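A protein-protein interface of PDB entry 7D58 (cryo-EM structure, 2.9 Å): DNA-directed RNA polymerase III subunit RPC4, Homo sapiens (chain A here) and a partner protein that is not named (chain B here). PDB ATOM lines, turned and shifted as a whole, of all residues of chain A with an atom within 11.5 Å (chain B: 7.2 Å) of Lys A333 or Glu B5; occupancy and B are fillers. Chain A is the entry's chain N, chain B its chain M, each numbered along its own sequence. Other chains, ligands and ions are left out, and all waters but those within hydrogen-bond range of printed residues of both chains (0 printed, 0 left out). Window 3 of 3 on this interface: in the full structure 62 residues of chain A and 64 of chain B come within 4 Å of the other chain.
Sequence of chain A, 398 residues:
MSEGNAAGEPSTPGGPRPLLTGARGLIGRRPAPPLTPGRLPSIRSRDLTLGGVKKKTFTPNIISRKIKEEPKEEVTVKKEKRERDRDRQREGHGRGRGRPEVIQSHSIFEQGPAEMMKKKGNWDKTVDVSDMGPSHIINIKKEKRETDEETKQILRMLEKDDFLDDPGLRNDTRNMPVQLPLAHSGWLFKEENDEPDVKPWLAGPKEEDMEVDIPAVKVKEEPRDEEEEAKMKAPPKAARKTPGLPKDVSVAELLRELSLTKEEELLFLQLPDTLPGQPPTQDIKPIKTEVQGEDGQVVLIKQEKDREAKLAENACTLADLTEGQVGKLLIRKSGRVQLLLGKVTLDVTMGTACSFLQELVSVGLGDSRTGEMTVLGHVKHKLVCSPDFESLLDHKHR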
ATOM      1  N   SER A 250      28.902 -26.941  -2.885  1.00  0.00           N
ATOM      2  CA  SER A 250      27.614 -26.299  -2.658  1.00  0.00           C
ATOM      3  C   SER A 250      27.334 -25.255  -3.732  1.00  0.00           C
ATOM      4  O   SER A 250      28.253 -24.744  -4.376  1.00  0.00           O
ATOM      5  CB  SER A 250      27.583 -25.647  -1.276  1.00  0.00           C
ATOM      6  OG  SER A 250      28.502 -24.570  -1.202  1.00  0.00           O
ATOM      7  N   ALA A 252      26.155 -22.222  -3.343  1.00  0.00           N
ATOM      8  CA  ALA A 252      26.642 -20.901  -2.954  1.00  0.00           C
ATOM      9  C   ALA A 252      28.117 -20.740  -3.294  1.00  0.00           C
ATOM     10  O   ALA A 252      28.501 -19.799  -4.000  1.00  0.00           O
ATOM     11  CB  ALA A 252      26.407 -20.669  -1.462  1.00  0.00           C
ATOM     12  N   GLU A 253      28.955 -21.653  -2.801  1.00  0.00           N
ATOM     13  CA  GLU A 253      30.377 -21.631  -3.129  1.00  0.00           C
ATOM     14  C   GLU A 253      30.590 -21.705  -4.636  1.00  0.00           C
ATOM     15  O   GLU A 253      31.450 -21.011  -5.192  1.00  0.00           O
ATOM     16  CB  GLU A 253      31.076 -22.793  -2.418  1.00  0.00           C
ATOM     17  CG  GLU A 253      32.532 -23.009  -2.785  1.00  0.00           C
ATOM     18  CD  GLU A 253      33.089 -24.293  -2.195  1.00  0.00           C
ATOM     19  OE1 GLU A 253      34.039 -24.217  -1.386  1.00  0.00           O
ATOM     20  OE2 GLU A 253      32.571 -25.377  -2.535  1.00  0.00           O
ATOM     21  N   ARG A 256      29.914 -18.509  -6.179  1.00  0.00           N
ATOM     22  CA  ARG A 256      30.940 -17.571  -5.730  1.00  0.00           C
ATOM     23  C   ARG A 256      32.199 -17.672  -6.582  1.00  0.00           C
ATOM     24  O   ARG A 256      32.710 -16.655  -7.070  1.00  0.00           O
ATOM     25  CB  ARG A 256      31.267 -17.813  -4.256  1.00  0.00           C
ATOM     26  CG  ARG A 256      30.243 -17.235  -3.290  1.00  0.00           C
ATOM     27  CD  ARG A 256      30.565 -17.608  -1.852  1.00  0.00           C
ATOM     28  NE  ARG A 256      29.507 -17.209  -0.926  1.00  0.00           N
ATOM     29  CZ  ARG A 256      29.551 -17.416   0.385  1.00  0.00           C
ATOM     30  NH1 ARG A 256      30.602 -18.019   0.925  1.00  0.00           N
ATOM     31  NH2 ARG A 256      28.547 -17.025   1.158  1.00  0.00           N
ATOM     32  N   LEU A 329      17.607 -13.666  -5.646  1.00  0.00           N
ATOM     33  CA  LEU A 329      18.359 -14.695  -4.937  1.00  0.00           C
ATOM     34  C   LEU A 329      18.980 -14.126  -3.669  1.00  0.00           C
ATOM     35  O   LEU A 329      19.421 -12.973  -3.639  1.00  0.00           O
ATOM     36  CB  LEU A 329      19.449 -15.296  -5.827  1.00  0.00           C
ATOM     37  CG  LEU A 329      19.084 -16.548  -6.631  1.00  0.00           C
ATOM     38  CD1 LEU A 329      18.831 -17.721  -5.693  1.00  0.00           C
ATOM     39  CD2 LEU A 329      17.874 -16.300  -7.513  1.00  0.00           C
ATOM     40  N   LEU A 330      19.012 -14.946  -2.622  1.00  0.00           N
ATOM     41  CA  LEU A 330      19.525 -14.554  -1.319  1.00  0.00           C
ATOM     42  C   LEU A 330      20.509 -15.616  -0.855  1.00  0.00           C
ATOM     43  O   LEU A 330      20.219 -16.814  -0.946  1.00  0.00           O
ATOM     44  CB  LEU A 330      18.389 -14.401  -0.297  1.00  0.00           C
ATOM     45  CG  LEU A 330      17.493 -13.154  -0.310  1.00  0.00           C
ATOM     46  CD1 LEU A 330      18.315 -11.883  -0.151  1.00  0.00           C
ATOM     47  CD2 LEU A 330      16.580 -13.086  -1.538  1.00  0.00           C
ATOM     48  N   ILE A 331      21.668 -15.181  -0.372  1.00  0.00           N
ATOM     49  CA  ILE A 331      22.707 -16.078   0.120  1.00  0.00           C
ATOM     50  C   ILE A 331      22.877 -15.812   1.609  1.00  0.00           C
ATOM     51  O   ILE A 331      23.353 -14.742   2.011  1.00  0.00           O
ATOM     52  CB  ILE A 331      24.027 -15.894  -0.638  1.00  0.00           C
ATOM     53  CG1 ILE A 331      23.820 -16.157  -2.132  1.00  0.00           C
ATOM     54  CG2 ILE A 331      25.101 -16.812  -0.071  1.00  0.00           C
ATOM     55  CD1 ILE A 331      25.033 -15.846  -2.981  1.00  0.00           C
ATOM     56  N   ARG A 332      22.491 -16.786   2.429  1.00  0.00           N
ATOM     57  CA  ARG A 332      22.521 -16.645   3.879  1.00  0.00           C
ATOM     58  C   ARG A 332      23.791 -17.272   4.442  1.00  0.00           C
ATOM     59  O   ARG A 332      24.269 -18.289   3.930  1.00  0.00           O
ATOM     60  CB  ARG A 332      21.286 -17.299   4.497  1.00  0.00           C
ATOM     61  CG  ARG A 332      19.961 -16.734   3.994  1.00  0.00           C
ATOM     62  CD  ARG A 332      19.745 -15.303   4.466  1.00  0.00           C
ATOM     63  NE  ARG A 332      18.441 -14.783   4.064  1.00  0.00           N
ATOM     64  CZ  ARG A 332      17.346 -14.851   4.814  1.00  0.00           C
ATOM     65  NH1 ARG A 332      17.397 -15.414   6.015  1.00  0.00           N
ATOM     66  NH2 ARG A 332      16.202 -14.353   4.369  1.00  0.00           N
ATOM     67  N   LYS A 333      24.333 -16.661   5.494  1.00  0.00           N
ATOM     68  CA  LYS A 333      25.536 -17.184   6.130  1.00  0.00           C
ATOM     69  C   LYS A 333      25.236 -18.490   6.858  1.00  0.00           C
ATOM     70  O   LYS A 333      24.264 -18.587   7.613  1.00  0.00           O
ATOM     71  CB  LYS A 333      26.107 -16.146   7.098  1.00  0.00           C
ATOM     72  CG  LYS A 333      26.950 -16.725   8.216  1.00  0.00           C
ATOM     73  CD  LYS A 333      27.366 -15.648   9.204  1.00  0.00           C
ATOM     74  CE  LYS A 333      28.026 -16.261  10.431  1.00  0.00           C
ATOM     75  NZ  LYS A 333      28.415 -15.229  11.431  1.00  0.00           N
ATOM     76  N   SER A 334      26.086 -19.492   6.623  1.00  0.00           N
ATOM     77  CA  SER A 334      25.945 -20.823   7.218  1.00  0.00           C
ATOM     78  C   SER A 334      24.578 -21.425   6.898  1.00  0.00           C
ATOM     79  O   SER A 334      23.951 -22.090   7.725  1.00  0.00           O
ATOM     80  CB  SER A 334      26.193 -20.783   8.727  1.00  0.00           C
ATOM     81  OG  SER A 334      25.128 -20.142   9.408  1.00  0.00           O
ATOM     82  N   GLY A 335      24.117 -21.182   5.674  1.00  0.00           N
ATOM     83  CA  GLY A 335      22.829 -21.680   5.240  1.00  0.00           C
ATOM     84  C   GLY A 335      22.839 -22.215   3.823  1.00  0.00           C
ATOM     85  O   GLY A 335      23.680 -23.047   3.467  1.00  0.00           O
ATOM     86  N   ARG A 336      21.909 -21.735   3.007  1.00  0.00           N
ATOM     87  CA  ARG A 336      21.743 -22.198   1.635  1.00  0.00           C
ATOM     88  C   ARG A 336      21.331 -21.003   0.783  1.00  0.00           C
ATOM     89  O   ARG A 336      21.256 -19.870   1.270  1.00  0.00           O
ATOM     90  CB  ARG A 336      20.718 -23.335   1.563  1.00  0.00           C
ATOM     91  CG  ARG A 336      19.288 -22.890   1.833  1.00  0.00           C
ATOM     92  CD  ARG A 336      18.989 -22.848   3.323  1.00  0.00           C
ATOM     93  NE  ARG A 336      17.595 -22.530   3.613  1.00  0.00           N
ATOM     94  CZ  ARG A 336      17.149 -22.178   4.814  1.00  0.00           C
ATOM     95  NH1 ARG A 336      17.990 -22.093   5.835  1.00  0.00           N
ATOM     96  NH2 ARG A 336      15.863 -21.907   4.995  1.00  0.00           N
ATOM     97  N   VAL A 337      21.053 -21.259  -0.492  1.00  0.00           N
ATOM     98  CA  VAL A 337      20.671 -20.209  -1.432  1.00  0.00           C
ATOM     99  C   VAL A 337      19.162 -20.274  -1.673  1.00  0.00           C
ATOM    100  O   VAL A 337      18.596 -21.337  -1.974  1.00  0.00           O
ATOM    101  CB  VAL A 337      21.483 -20.296  -2.730  1.00  0.00           C
ATOM    102  CG1 VAL A 337      22.940 -19.995  -2.437  1.00  0.00           C
ATOM    103  CG2 VAL A 337      21.420 -21.689  -3.294  1.00  0.00           C
ATOM    104  N   GLN A 338      18.516 -19.110  -1.543  1.00  0.00           N
ATOM    105  CA  GLN A 338      17.085 -18.981  -1.288  1.00  0.00           C
ATOM    106  C   GLN A 338      16.488 -18.013  -2.306  1.00  0.00           C
ATOM    107  O   GLN A 338      16.893 -16.850  -2.378  1.00  0.00           O
ATOM    108  CB  GLN A 338      16.880 -18.488   0.143  1.00  0.00           C
ATOM    109  CG  GLN A 338      15.470 -18.522   0.688  1.00  0.00           C
ATOM    110  CD  GLN A 338      15.436 -18.091   2.144  1.00  0.00           C
ATOM    111  OE1 GLN A 338      16.460 -17.699   2.706  1.00  0.00           O
ATOM    112  NE2 GLN A 338      14.268 -18.173   2.764  1.00  0.00           N
ATOM    113  N   ASN B   3      18.375 -17.638  14.646  1.00  0.00           N
ATOM    114  CA  ASN B   3      18.020 -17.515  13.237  1.00  0.00           C
ATOM    115  C   ASN B   3      18.394 -16.138  12.701  1.00  0.00           C
ATOM    116  O   ASN B   3      18.428 -15.923  11.489  1.00  0.00           O
ATOM    117  CB  ASN B   3      16.524 -17.772  13.033  1.00  0.00           C
ATOM    118  CG  ASN B   3      15.652 -16.707  13.680  1.00  0.00           C
ATOM    119  OD1 ASN B   3      15.572 -15.575  13.202  1.00  0.00           O
ATOM    120  ND2 ASN B   3      14.997 -17.068  14.778  1.00  0.00           N
ATOM    121  N   GLU B   4      18.675 -15.204  13.608  1.00  0.00           N
ATOM    122  CA  GLU B   4      18.984 -13.835  13.220  1.00  0.00           C
ATOM    123  C   GLU B   4      20.401 -13.670  12.689  1.00  0.00           C
ATOM    124  O   GLU B   4      20.759 -12.567  12.262  1.00  0.00           O
ATOM    125  CB  GLU B   4      18.773 -12.884  14.403  1.00  0.00           C
ATOM    126  CG  GLU B   4      17.337 -12.822  14.893  1.00  0.00           C
ATOM    127  CD  GLU B   4      16.376 -12.279  13.847  1.00  0.00           C
ATOM    128  OE1 GLU B   4      16.792 -11.433  13.028  1.00  0.00           O
ATOM    129  OE2 GLU B   4      15.201 -12.707  13.847  1.00  0.00           O
ATOM    130  N   GLU B   5      21.207 -14.731  12.695  1.00  0.00           N
ATOM    131  CA  GLU B   5      22.560 -14.699  12.155  1.00  0.00           C
ATOM    132  C   GLU B   5      22.575 -14.669  10.630  1.00  0.00           C
ATOM    133  O   GLU B   5      23.648 -14.749  10.023  1.00  0.00           O
ATOM    134  CB  GLU B   5      23.361 -15.895  12.671  1.00  0.00           C
ATOM    135  CG  GLU B   5      23.067 -17.211  11.959  1.00  0.00           C
ATOM    136  CD  GLU B   5      21.721 -17.795  12.338  1.00  0.00           C
ATOM    137  OE1 GLU B   5      21.150 -18.557  11.531  1.00  0.00           O
ATOM    138  OE2 GLU B   5      21.236 -17.491  13.449  1.00  0.00           O
ATOM    139  N   ASP B   6      21.405 -14.550  10.003  1.00  0.00           N
ATOM    140  CA  ASP B   6      21.281 -14.524   8.553  1.00  0.00           C
ATOM    141  C   ASP B   6      21.102 -13.119   7.997  1.00  0.00           C
ATOM    142  O   ASP B   6      21.058 -12.954   6.773  1.00  0.00           O
ATOM    143  CB  ASP B   6      20.105 -15.403   8.112  1.00  0.00           C
ATOM    144  CG  ASP B   6      20.482 -16.863   8.002  1.00  0.00           C
ATOM    145  OD1 ASP B   6      21.461 -17.272   8.661  1.00  0.00           O
ATOM    146  OD2 ASP B   6      19.801 -17.600   7.260  1.00  0.00           O
ATOM    147  N   ASP B   7      20.996 -12.108   8.857  1.00  0.00           N
ATOM    148  CA  ASP B   7      20.782 -10.723   8.450  1.00  0.00           C
ATOM    149  C   ASP B   7      22.040 -10.060   7.889  1.00  0.00           C
ATOM    150  O   ASP B   7      21.971  -9.460   6.808  1.00  0.00           O
ATOM    151  CB  ASP B   7      20.256  -9.894   9.626  1.00  0.00           C
ATOM    152  CG  ASP B   7      18.856 -10.280  10.039  1.00  0.00           C
ATOM    153  OD1 ASP B   7      18.073 -10.718   9.170  1.00  0.00           O
ATOM    154  OD2 ASP B   7      18.541 -10.142  11.239  1.00  0.00           O
ATOM    155  N   PRO B   8      23.207 -10.104   8.592  1.00  0.00           N
ATOM    156  CA  PRO B   8      24.383  -9.379   8.086  1.00  0.00           C
ATOM    157  C   PRO B   8      24.833  -9.821   6.701  1.00  0.00           C
ATOM    158  O   PRO B   8      24.898  -8.998   5.782  1.00  0.00           O
ATOM    159  CB  PRO B   8      25.460  -9.683   9.139  1.00  0.00           C
ATOM    160  CG  PRO B   8      24.700  -9.984  10.370  1.00  0.00           C
ATOM    161  CD  PRO B   8      23.500 -10.739   9.890  1.00  0.00           C
ATOM    162  N   VAL B   9      25.134 -11.105   6.530  1.00  0.00           N
ATOM    163  CA  VAL B   9      25.612 -11.638   5.259  1.00  0.00           C
ATOM    164  C   VAL B   9      24.383 -11.936   4.408  1.00  0.00           C
ATOM    165  O   VAL B   9      23.732 -12.970   4.575  1.00  0.00           O
ATOM    166  CB  VAL B   9      26.480 -12.882   5.450  1.00  0.00           C
ATOM    167  CG1 VAL B   9      27.219 -13.220   4.157  1.00  0.00           C
ATOM    168  CG2 VAL B   9      27.453 -12.674   6.595  1.00  0.00           C
ATOM    169  N   VAL B  10      24.069 -11.030   3.484  1.00  0.00           N
ATOM    170  CA  VAL B  10      22.924 -11.177   2.589  1.00  0.00           C
ATOM    171  C   VAL B  10      23.365 -10.738   1.201  1.00  0.00           C
ATOM    172  O   VAL B  10      23.665  -9.557   0.985  1.00  0.00           O
ATOM    173  CB  VAL B  10      21.707 -10.367   3.057  1.00  0.00           C
ATOM    174  CG1 VAL B  10      20.704 -10.207   1.919  1.00  0.00           C
ATOM    175  CG2 VAL B  10      21.049 -11.039   4.245  1.00  0.00           C
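The side-chain carboxylate (OD2) of Asp B6 is in salt-bridge range of the guanidinium group (NH1) of Arg A332, at 3.5 Å.
O of Ile A331 sits close to O of Val B9 (3.1 Å).
The backbone carbonyl oxygen (O) of Lys A333 lies close to the side-chain carboxylate (OD1) of Asp B6 (3.3 Å).
Hydrophobic or aromatic side chains of chain B that line the printed part of chain A: Val B9 and Val B10.
Hydrophobic or aromatic side chains of chain A within 4 Å of the printed part of chain B: Leu A330.
Among the printed residues, 8 pairs touch across the chains.
Among the printed residues, Asp or Glu carboxylates within 4 Å of a Lys or Arg side-chain nitrogen of the other chain: Arg A332 with Asp B6 (3.5 Å).
Among the printed residues, merely in contact across the chains: Leu A330 with Val B10 (3.6 Å), Ile A331 with Val B10 (3.6 Å), Lys A333 with Val B9 (3.7 Å), Lys A333 with Glu B5 (3.9 Å) and Arg A332 with Val B9 (3.9 Å).
The backbone NH (N) of Asn B3 lies within hydrogen-bond range of the side-chain carboxylate (OE2) of Glu B5, 3.1 Å away.
N of Leu A330 sits at hydrogen-bond distance from O of Gln A338 (2.9 Å).
Lys A333 touches three residues of chain B.
Glu B5 touches just one residue of chain A: Lys A333.
No residue of chain A comes within 4 Å of Asn B3.
Asp B6 touches just these residues of chain A: Arg A332 and Lys A333.
No residue of chain A comes within 4 Å of Asp B7.
No residue of chain A comes within 4 Å of Pro B8.
Val B9 touches three residues of chain A.
Printed residues of chain B within 4 Å of Leu A330: Val B10.
Of the printed residues of chain B, Arg A332 touches Asp B6 (3.2 Å) and Val B9 (3.9 Å).
Printed residues of chain B within 4 Å of Ile A331: Val B9 (3.1 Å) and Val B10 (3.6 Å).
Of the printed residues of chain A, Val B10 touches Leu A330 and Ile A331.
Arg A336 touches none of the printed residues of chain B.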
